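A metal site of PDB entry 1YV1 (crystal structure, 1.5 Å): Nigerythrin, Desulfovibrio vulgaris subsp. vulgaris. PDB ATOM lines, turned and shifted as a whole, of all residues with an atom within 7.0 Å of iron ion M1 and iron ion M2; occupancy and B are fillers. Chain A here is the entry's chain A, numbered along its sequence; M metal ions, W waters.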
ATOM      1  N   ALA A  36      -3.858  16.004 -25.357  1.00  0.00           N
ATOM      2  CA  ALA A  36      -4.891  16.706 -24.600  1.00  0.00           C
ATOM      3  C   ALA A  36      -4.268  17.876 -23.841  1.00  0.00           C
ATOM      4  O   ALA A  36      -4.803  18.978 -23.838  1.00  0.00           O
ATOM      5  CB  ALA A  36      -5.586  15.749 -23.656  1.00  0.00           C
ATOM      6  N   GLY A  39      -3.595  20.690 -26.087  1.00  0.00           N
ATOM      7  CA  GLY A  39      -4.835  21.372 -26.402  1.00  0.00           C
ATOM      8  C   GLY A  39      -5.335  22.227 -25.250  1.00  0.00           C
ATOM      9  O   GLY A  39      -5.817  23.342 -25.452  1.00  0.00           O
ATOM     10  N   GLU A  40      -5.216  21.691 -24.039  1.00  0.00           N
ATOM     11  CA  GLU A  40      -5.646  22.391 -22.838  1.00  0.00           C
ATOM     12  C   GLU A  40      -4.791  23.640 -22.629  1.00  0.00           C
ATOM     13  O   GLU A  40      -5.293  24.692 -22.210  1.00  0.00           O
ATOM     14  CB  GLU A  40      -5.552  21.489 -21.600  1.00  0.00           C
ATOM     15  CG  GLU A  40      -6.478  20.299 -21.611  1.00  0.00           C
ATOM     16  CD  GLU A  40      -7.896  20.700 -21.236  1.00  0.00           C
ATOM     17  OE1 GLU A  40      -8.069  21.797 -20.677  1.00  0.00           O
ATOM     18  OE2 GLU A  40      -8.819  19.902 -21.491  1.00  0.00           O
ATOM     19  N   ALA A  43      -5.913  26.178 -24.951  1.00  0.00           N
ATOM     20  CA  ALA A  43      -7.181  26.733 -24.500  1.00  0.00           C
ATOM     21  C   ALA A  43      -6.968  27.754 -23.386  1.00  0.00           C
ATOM     22  O   ALA A  43      -7.583  28.819 -23.381  1.00  0.00           O
ATOM     23  CB  ALA A  43      -8.107  25.612 -24.011  1.00  0.00           C
ATOM     24  N   TYR A  47      -8.174  31.561 -23.696  1.00  0.00           N
ATOM     25  CA  TYR A  47      -9.113  32.194 -22.779  1.00  0.00           C
ATOM     26  C   TYR A  47      -8.487  33.328 -21.990  1.00  0.00           C
ATOM     27  O   TYR A  47      -9.174  34.303 -21.664  1.00  0.00           O
ATOM     28  CB  TYR A  47      -9.705  31.120 -21.852  1.00  0.00           C
ATOM     29  CG  TYR A  47     -10.494  30.070 -22.610  1.00  0.00           C
ATOM     30  CD1 TYR A  47     -10.795  28.834 -22.028  1.00  0.00           C
ATOM     31  CD2 TYR A  47     -10.953  30.315 -23.904  1.00  0.00           C
ATOM     32  CE1 TYR A  47     -11.526  27.875 -22.725  1.00  0.00           C
ATOM     33  CE2 TYR A  47     -11.692  29.360 -24.606  1.00  0.00           C
ATOM     34  CZ  TYR A  47     -11.967  28.146 -24.010  1.00  0.00           C
ATOM     35  OH  TYR A  47     -12.687  27.205 -24.714  1.00  0.00           O
ATOM     36  N   THR A  69     -12.945  29.925 -16.902  1.00  0.00           N
ATOM     37  CA  THR A  69     -12.777  28.788 -17.802  1.00  0.00           C
ATOM     38  C   THR A  69     -11.290  28.506 -18.018  1.00  0.00           C
ATOM     39  O   THR A  69     -10.897  27.357 -18.140  1.00  0.00           O
ATOM     40  CB  THR A  69     -13.479  29.045 -19.141  1.00  0.00           C
ATOM     41  OG1 THR A  69     -14.824  29.487 -18.890  1.00  0.00           O
ATOM     42  CG2 THR A  69     -13.550  27.748 -19.969  1.00  0.00           C
ATOM     43  N   ALA A  72     -10.278  26.541 -15.299  1.00  0.00           N
ATOM     44  CA  ALA A  72     -10.815  25.188 -15.440  1.00  0.00           C
ATOM     45  C   ALA A  72      -9.882  24.338 -16.289  1.00  0.00           C
ATOM     46  O   ALA A  72      -9.643  23.169 -15.983  1.00  0.00           O
ATOM     47  CB  ALA A  72     -12.201  25.239 -16.068  1.00  0.00           C
ATOM     48  N   GLU A  73      -9.341  24.924 -17.357  1.00  0.00           N
ATOM     49  CA  GLU A  73      -8.446  24.163 -18.228  1.00  0.00           C
ATOM     50  C   GLU A  73      -7.149  23.846 -17.495  1.00  0.00           C
ATOM     51  O   GLU A  73      -6.510  22.818 -17.761  1.00  0.00           O
ATOM     52  CB  GLU A  73      -8.173  24.945 -19.519  1.00  0.00           C
ATOM     53  CG  GLU A  73      -9.415  25.564 -20.171  1.00  0.00           C
ATOM     54  CD  GLU A  73     -10.593  24.602 -20.352  1.00  0.00           C
ATOM     55  OE1 GLU A  73     -10.474  23.419 -19.930  1.00  0.00           O
ATOM     56  OE2 GLU A  73     -11.614  25.002 -20.936  1.00  0.00           O
ATOM     57  N   LEU A  74      -6.753  24.716 -16.557  1.00  0.00           N
ATOM     58  CA  LEU A  74      -5.532  24.475 -15.797  1.00  0.00           C
ATOM     59  C   LEU A  74      -5.746  23.264 -14.892  1.00  0.00           C
ATOM     60  O   LEU A  74      -4.818  22.510 -14.609  1.00  0.00           O
ATOM     61  CB  LEU A  74      -5.190  25.711 -14.959  1.00  0.00           C
ATOM     62  CG  LEU A  74      -3.786  25.796 -14.371  1.00  0.00           C
ATOM     63  CD1 LEU A  74      -2.742  25.609 -15.464  1.00  0.00           C
ATOM     64  CD2 LEU A  74      -3.605  27.142 -13.681  1.00  0.00           C
ATOM     65  N   ILE A  75      -6.989  23.081 -14.447  1.00  0.00           N
ATOM     66  CA  ILE A  75      -7.336  21.952 -13.598  1.00  0.00           C
ATOM     67  C   ILE A  75      -7.212  20.675 -14.439  1.00  0.00           C
ATOM     68  O   ILE A  75      -6.683  19.658 -13.982  1.00  0.00           O
ATOM     69  CB  ILE A  75      -8.789  22.076 -13.071  1.00  0.00           C
ATOM     70  CG1 ILE A  75      -8.860  23.223 -12.065  1.00  0.00           C
ATOM     71  CG2 ILE A  75      -9.238  20.769 -12.442  1.00  0.00           C
ATOM     72  CD1 ILE A  75     -10.280  23.578 -11.638  1.00  0.00           C
ATOM     73  N   HIS A  76      -7.694  20.733 -15.678  1.00  0.00           N
ATOM     74  CA  HIS A  76      -7.613  19.581 -16.570  1.00  0.00           C
ATOM     75  C   HIS A  76      -6.164  19.224 -16.850  1.00  0.00           C
ATOM     76  O   HIS A  76      -5.802  18.055 -16.881  1.00  0.00           O
ATOM     77  CB  HIS A  76      -8.352  19.891 -17.879  1.00  0.00           C
ATOM     78  CG  HIS A  76      -9.822  20.105 -17.692  1.00  0.00           C
ATOM     79  ND1 HIS A  76     -10.619  20.688 -18.654  1.00  0.00           N
ATOM     80  CD2 HIS A  76     -10.630  19.824 -16.647  1.00  0.00           C
ATOM     81  CE1 HIS A  76     -11.862  20.769 -18.204  1.00  0.00           C
ATOM     82  NE2 HIS A  76     -11.889  20.250 -16.991  1.00  0.00           N
ATOM     83  N   ILE A  77      -5.335  20.244 -17.044  1.00  0.00           N
ATOM     84  CA  ILE A  77      -3.905  20.038 -17.281  1.00  0.00           C
ATOM     85  C   ILE A  77      -3.282  19.321 -16.080  1.00  0.00           C
ATOM     86  O   ILE A  77      -2.475  18.407 -16.244  1.00  0.00           O
ATOM     87  CB  ILE A  77      -3.177  21.371 -17.515  1.00  0.00           C
ATOM     88  CG1 ILE A  77      -3.611  21.974 -18.858  1.00  0.00           C
ATOM     89  CG2 ILE A  77      -1.667  21.166 -17.490  1.00  0.00           C
ATOM     90  CD1 ILE A  77      -3.156  23.399 -19.083  1.00  0.00           C
ATOM     91  N   GLU A  80      -4.299  15.577 -16.102  1.00  0.00           N
ATOM     92  CA  GLU A  80      -3.654  14.835 -17.177  1.00  0.00           C
ATOM     93  C   GLU A  80      -2.142  14.751 -16.988  1.00  0.00           C
ATOM     94  O   GLU A  80      -1.530  13.723 -17.270  1.00  0.00           O
ATOM     95  CB  GLU A  80      -4.011  15.484 -18.513  1.00  0.00           C
ATOM     96  CG  GLU A  80      -5.529  15.599 -18.675  1.00  0.00           C
ATOM     97  CD  GLU A  80      -5.968  16.353 -19.920  1.00  0.00           C
ATOM     98  OE1 GLU A  80      -5.229  17.220 -20.413  1.00  0.00           O
ATOM     99  OE2 GLU A  80      -7.097  16.079 -20.387  1.00  0.00           O
ATOM    100  N   GLY A 111     -14.601  30.045 -28.519  1.00  0.00           N
ATOM    101  CA  GLY A 111     -14.495  29.218 -27.330  1.00  0.00           C
ATOM    102  C   GLY A 111     -15.481  28.062 -27.382  1.00  0.00           C
ATOM    103  O   GLY A 111     -15.096  26.916 -27.166  1.00  0.00           O
ATOM    104  N   GLY A 114     -14.462  25.261 -29.763  1.00  0.00           N
ATOM    105  CA  GLY A 114     -13.397  24.399 -29.276  1.00  0.00           C
ATOM    106  C   GLY A 114     -13.913  23.426 -28.230  1.00  0.00           C
ATOM    107  O   GLY A 114     -13.561  22.247 -28.232  1.00  0.00           O
ATOM    108  N   GLU A 115     -14.752  23.932 -27.331  1.00  0.00           N
ATOM    109  CA  GLU A 115     -15.345  23.122 -26.281  1.00  0.00           C
ATOM    110  C   GLU A 115     -16.157  21.981 -26.889  1.00  0.00           C
ATOM    111  O   GLU A 115     -16.097  20.846 -26.426  1.00  0.00           O
ATOM    112  CB  GLU A 115     -16.273  23.968 -25.405  1.00  0.00           C
ATOM    113  CG  GLU A 115     -15.600  25.138 -24.721  1.00  0.00           C
ATOM    114  CD  GLU A 115     -14.642  24.731 -23.608  1.00  0.00           C
ATOM    115  OE1 GLU A 115     -14.631  23.545 -23.217  1.00  0.00           O
ATOM    116  OE2 GLU A 115     -13.883  25.604 -23.120  1.00  0.00           O
ATOM    117  N   GLU A 118     -13.906  19.276 -28.304  1.00  0.00           N
ATOM    118  CA  GLU A 118     -13.327  18.462 -27.249  1.00  0.00           C
ATOM    119  C   GLU A 118     -14.321  17.507 -26.597  1.00  0.00           C
ATOM    120  O   GLU A 118     -13.982  16.358 -26.314  1.00  0.00           O
ATOM    121  CB  GLU A 118     -12.709  19.361 -26.190  1.00  0.00           C
ATOM    122  CG  GLU A 118     -11.574  20.224 -26.709  1.00  0.00           C
ATOM    123  CD  GLU A 118     -11.372  21.488 -25.890  1.00  0.00           C
ATOM    124  OE1 GLU A 118     -10.457  22.280 -26.218  1.00  0.00           O
ATOM    125  OE2 GLU A 118     -12.146  21.690 -24.927  1.00  0.00           O
ATOM    126  N   TYR A 123     -12.144  14.152 -26.695  1.00  0.00           N
ATOM    127  CA  TYR A 123     -12.202  13.356 -25.469  1.00  0.00           C
ATOM    128  C   TYR A 123     -12.917  12.010 -25.604  1.00  0.00           C
ATOM    129  O   TYR A 123     -12.458  11.020 -25.064  1.00  0.00           O
ATOM    130  CB  TYR A 123     -12.726  14.197 -24.307  1.00  0.00           C
ATOM    131  CG  TYR A 123     -11.641  15.090 -23.726  1.00  0.00           C
ATOM    132  CD1 TYR A 123     -11.826  16.463 -23.572  1.00  0.00           C
ATOM    133  CD2 TYR A 123     -10.401  14.550 -23.345  1.00  0.00           C
ATOM    134  CE1 TYR A 123     -10.804  17.277 -23.057  1.00  0.00           C
ATOM    135  CE2 TYR A 123      -9.389  15.348 -22.845  1.00  0.00           C
ATOM    136  CZ  TYR A 123      -9.588  16.705 -22.699  1.00  0.00           C
ATOM    137  OH  TYR A 123      -8.579  17.493 -22.200  1.00  0.00           O
ATOM    138  N   ALA A 145     -12.797  15.805 -17.846  1.00  0.00           N
ATOM    139  CA  ALA A 145     -12.532  16.923 -18.733  1.00  0.00           C
ATOM    140  C   ALA A 145     -13.669  17.033 -19.756  1.00  0.00           C
ATOM    141  O   ALA A 145     -14.212  18.105 -19.968  1.00  0.00           O
ATOM    142  CB  ALA A 145     -11.199  16.730 -19.445  1.00  0.00           C
ATOM    143  N   LYS A 146     -14.015  15.904 -20.373  1.00  0.00           N
ATOM    144  CA  LYS A 146     -15.085  15.841 -21.371  1.00  0.00           C
ATOM    145  C   LYS A 146     -16.389  16.457 -20.867  1.00  0.00           C
ATOM    146  O   LYS A 146     -17.015  17.253 -21.559  1.00  0.00           O
ATOM    147  CB  LYS A 146     -15.310  14.389 -21.793  1.00  0.00           C
ATOM    148  CG  LYS A 146     -16.461  14.128 -22.771  1.00  0.00           C
ATOM    149  CD  LYS A 146     -17.791  13.925 -22.035  1.00  0.00           C
ATOM    150  CE  LYS A 146     -18.903  13.446 -22.976  1.00  0.00           C
ATOM    151  NZ  LYS A 146     -19.336  14.481 -23.966  1.00  0.00           N
ATOM    152  N   ALA A 148     -16.797  18.554 -18.382  1.00  0.00           N
ATOM    153  CA  ALA A 148     -16.639  19.967 -18.092  1.00  0.00           C
ATOM    154  C   ALA A 148     -16.679  20.822 -19.362  1.00  0.00           C
ATOM    155  O   ALA A 148     -17.258  21.907 -19.361  1.00  0.00           O
ATOM    156  CB  ALA A 148     -15.325  20.206 -17.353  1.00  0.00           C
ATOM    157  N   GLU A 149     -16.107  20.317 -20.450  1.00  0.00           N
ATOM    158  CA  GLU A 149     -16.077  21.082 -21.690  1.00  0.00           C
ATOM    159  C   GLU A 149     -17.474  21.363 -22.257  1.00  0.00           C
ATOM    160  O   GLU A 149     -17.719  22.459 -22.770  1.00  0.00           O
ATOM    161  CB  GLU A 149     -15.243  20.361 -22.769  1.00  0.00           C
ATOM    162  CG  GLU A 149     -13.953  19.748 -22.242  1.00  0.00           C
ATOM    163  CD  GLU A 149     -12.953  20.733 -21.665  1.00  0.00           C
ATOM    164  OE1 GLU A 149     -13.360  21.828 -21.251  1.00  0.00           O
ATOM    165  OE2 GLU A 149     -11.753  20.397 -21.616  1.00  0.00           O
ATOM    166  N   SER A 150     -18.395  20.406 -22.173  1.00  0.00           N
ATOM    167  CA  SER A 150     -19.730  20.673 -22.688  1.00  0.00           C
ATOM    168  C   SER A 150     -20.433  21.720 -21.838  1.00  0.00           C
ATOM    169  O   SER A 150     -21.250  22.488 -22.337  1.00  0.00           O
ATOM    170  CB  SER A 150     -20.558  19.383 -22.792  1.00  0.00           C
ATOM    171  OG  SER A 150     -20.691  18.729 -21.559  1.00  0.00           O
ATOM    172  N   HIS A 152     -18.808  24.189 -20.358  1.00  0.00           N
ATOM    173  CA  HIS A 152     -18.161  25.421 -20.797  1.00  0.00           C
ATOM    174  C   HIS A 152     -18.824  25.946 -22.072  1.00  0.00           C
ATOM    175  O   HIS A 152     -19.058  27.151 -22.213  1.00  0.00           O
ATOM    176  CB  HIS A 152     -16.705  25.210 -21.076  1.00  0.00           C
ATOM    177  CG  HIS A 152     -15.892  24.788 -19.850  1.00  0.00           C
ATOM    178  ND1 HIS A 152     -14.616  24.290 -19.936  1.00  0.00           N
ATOM    179  CD2 HIS A 152     -16.210  24.814 -18.538  1.00  0.00           C
ATOM    180  CE1 HIS A 152     -14.172  24.024 -18.709  1.00  0.00           C
ATOM    181  NE2 HIS A 152     -15.129  24.330 -17.848  1.00  0.00           N
ATOM    182  N   ALA A 153     -19.120  25.041 -22.990  1.00  0.00           N
ATOM    183  CA  ALA A 153     -19.757  25.417 -24.243  1.00  0.00           C
ATOM    184  C   ALA A 153     -21.091  26.109 -23.991  1.00  0.00           C
ATOM    185  O   ALA A 153     -21.377  27.151 -24.571  1.00  0.00           O
ATOM    186  CB  ALA A 153     -19.971  24.184 -25.120  1.00  0.00           C
ATOM    187  N   TYR A 156     -20.651  29.587 -22.558  1.00  0.00           N
ATOM    188  CA  TYR A 156     -20.224  30.546 -23.573  1.00  0.00           C
ATOM    189  C   TYR A 156     -21.403  30.985 -24.449  1.00  0.00           C
ATOM    190  O   TYR A 156     -21.521  32.160 -24.799  1.00  0.00           O
ATOM    191  CB  TYR A 156     -19.101  29.939 -24.427  1.00  0.00           C
ATOM    192  CG  TYR A 156     -17.735  29.966 -23.762  1.00  0.00           C
ATOM    193  CD1 TYR A 156     -16.768  29.014 -24.094  1.00  0.00           C
ATOM    194  CD2 TYR A 156     -17.396  30.963 -22.851  1.00  0.00           C
ATOM    195  CE1 TYR A 156     -15.488  29.068 -23.531  1.00  0.00           C
ATOM    196  CE2 TYR A 156     -16.112  31.027 -22.288  1.00  0.00           C
ATOM    197  CZ  TYR A 156     -15.165  30.072 -22.631  1.00  0.00           C
ATOM    198  OH  TYR A 156     -13.896  30.153 -22.091  1.00  0.00           O
ATOM    199  N   CYS A 177     -13.011  19.156 -11.036  1.00  0.00           N
ATOM    200  CA  CYS A 177     -13.250  18.828 -12.435  1.00  0.00           C
ATOM    201  C   CYS A 177     -13.354  19.994 -13.402  1.00  0.00           C
ATOM    202  O   CYS A 177     -13.404  19.786 -14.614  1.00  0.00           O
ATOM    203  CB  CYS A 177     -14.521  17.985 -12.535  1.00  0.00           C
ATOM    204  SG  CYS A 177     -16.022  18.902 -12.163  1.00  0.00           S
ATOM    205  N   GLY A 178     -13.408  21.214 -12.890  1.00  0.00           N
ATOM    206  CA  GLY A 178     -13.506  22.350 -13.790  1.00  0.00           C
ATOM    207  C   GLY A 178     -14.916  22.764 -14.144  1.00  0.00           C
ATOM    208  O   GLY A 178     -15.121  23.595 -15.028  1.00  0.00           O
HETATM  209 FE    FE M   1     -13.171  23.897 -21.620  1.00  0.00          FE
HETATM  210 FE    FE M   2     -10.298  21.455 -20.635  1.00  0.00          FE
HETATM  211  O   HOH W   1      -9.944  22.212 -22.843  1.00  0.00           O
HETATM  212  O   HOH W   2     -11.781  23.764 -23.391  1.00  0.00           O
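The side-chain carboxylate (OE2) of Glu 40 sits close to the side-chain hydroxyl (OH) of Tyr 123 (2.5 Å). The side-chain hydroxyl of Tyr 47 lies close to the side-chain carboxylate of Glu 115, 2.6 Å away. A ring nitrogen (NE2) of His 152 sits at hydrogen-bond distance from the backbone carbonyl oxygen (O) of Gly 178, at 2.9 Å. NE2 of His 76 is in hydrogen-bond range of O of Cys 177, 2.9 Å away.
Four residues have an atom within 4 Å of iron ion M1: Glu 73, Glu 115, Glu 149 and His 152.
Within 4 Å of iron ion M2: Glu 40, Glu 73, His 76 and Glu 149.
Iron ion M1 is bound by OE2 of Glu 73 (2.0 Å). The side-chain carboxylate (OE1) of Glu 149 binds iron ion M1, at 2.1 Å. OE1 of Glu 115 binds iron ion M1 (2.2 Å). A ring nitrogen (ND1) of His 152 is bound to iron ion M1 (2.3 Å). Water W2 is bound to iron ion M1, 2.3 Å away. Iron ion M1 is bound by the side-chain carboxylate (OE2) of Glu 115, 2.4 Å away.
Iron ion M2 is bound by OE2 of Glu 149. OE1 of Glu 73 is bound to iron ion M2. Iron ion M2 is bound by ND1 of His 76, at 2.1 Å. OE1 of Glu 40 binds iron ion M2, at 2.3 Å. The side-chain carboxylate (OE2) of Glu 40 is bound to iron ion M2 (2.3 Å). Water W1 is bound to iron ion M2 (2.4 Å). Iron ion M2 has six donor atoms within binding distance.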
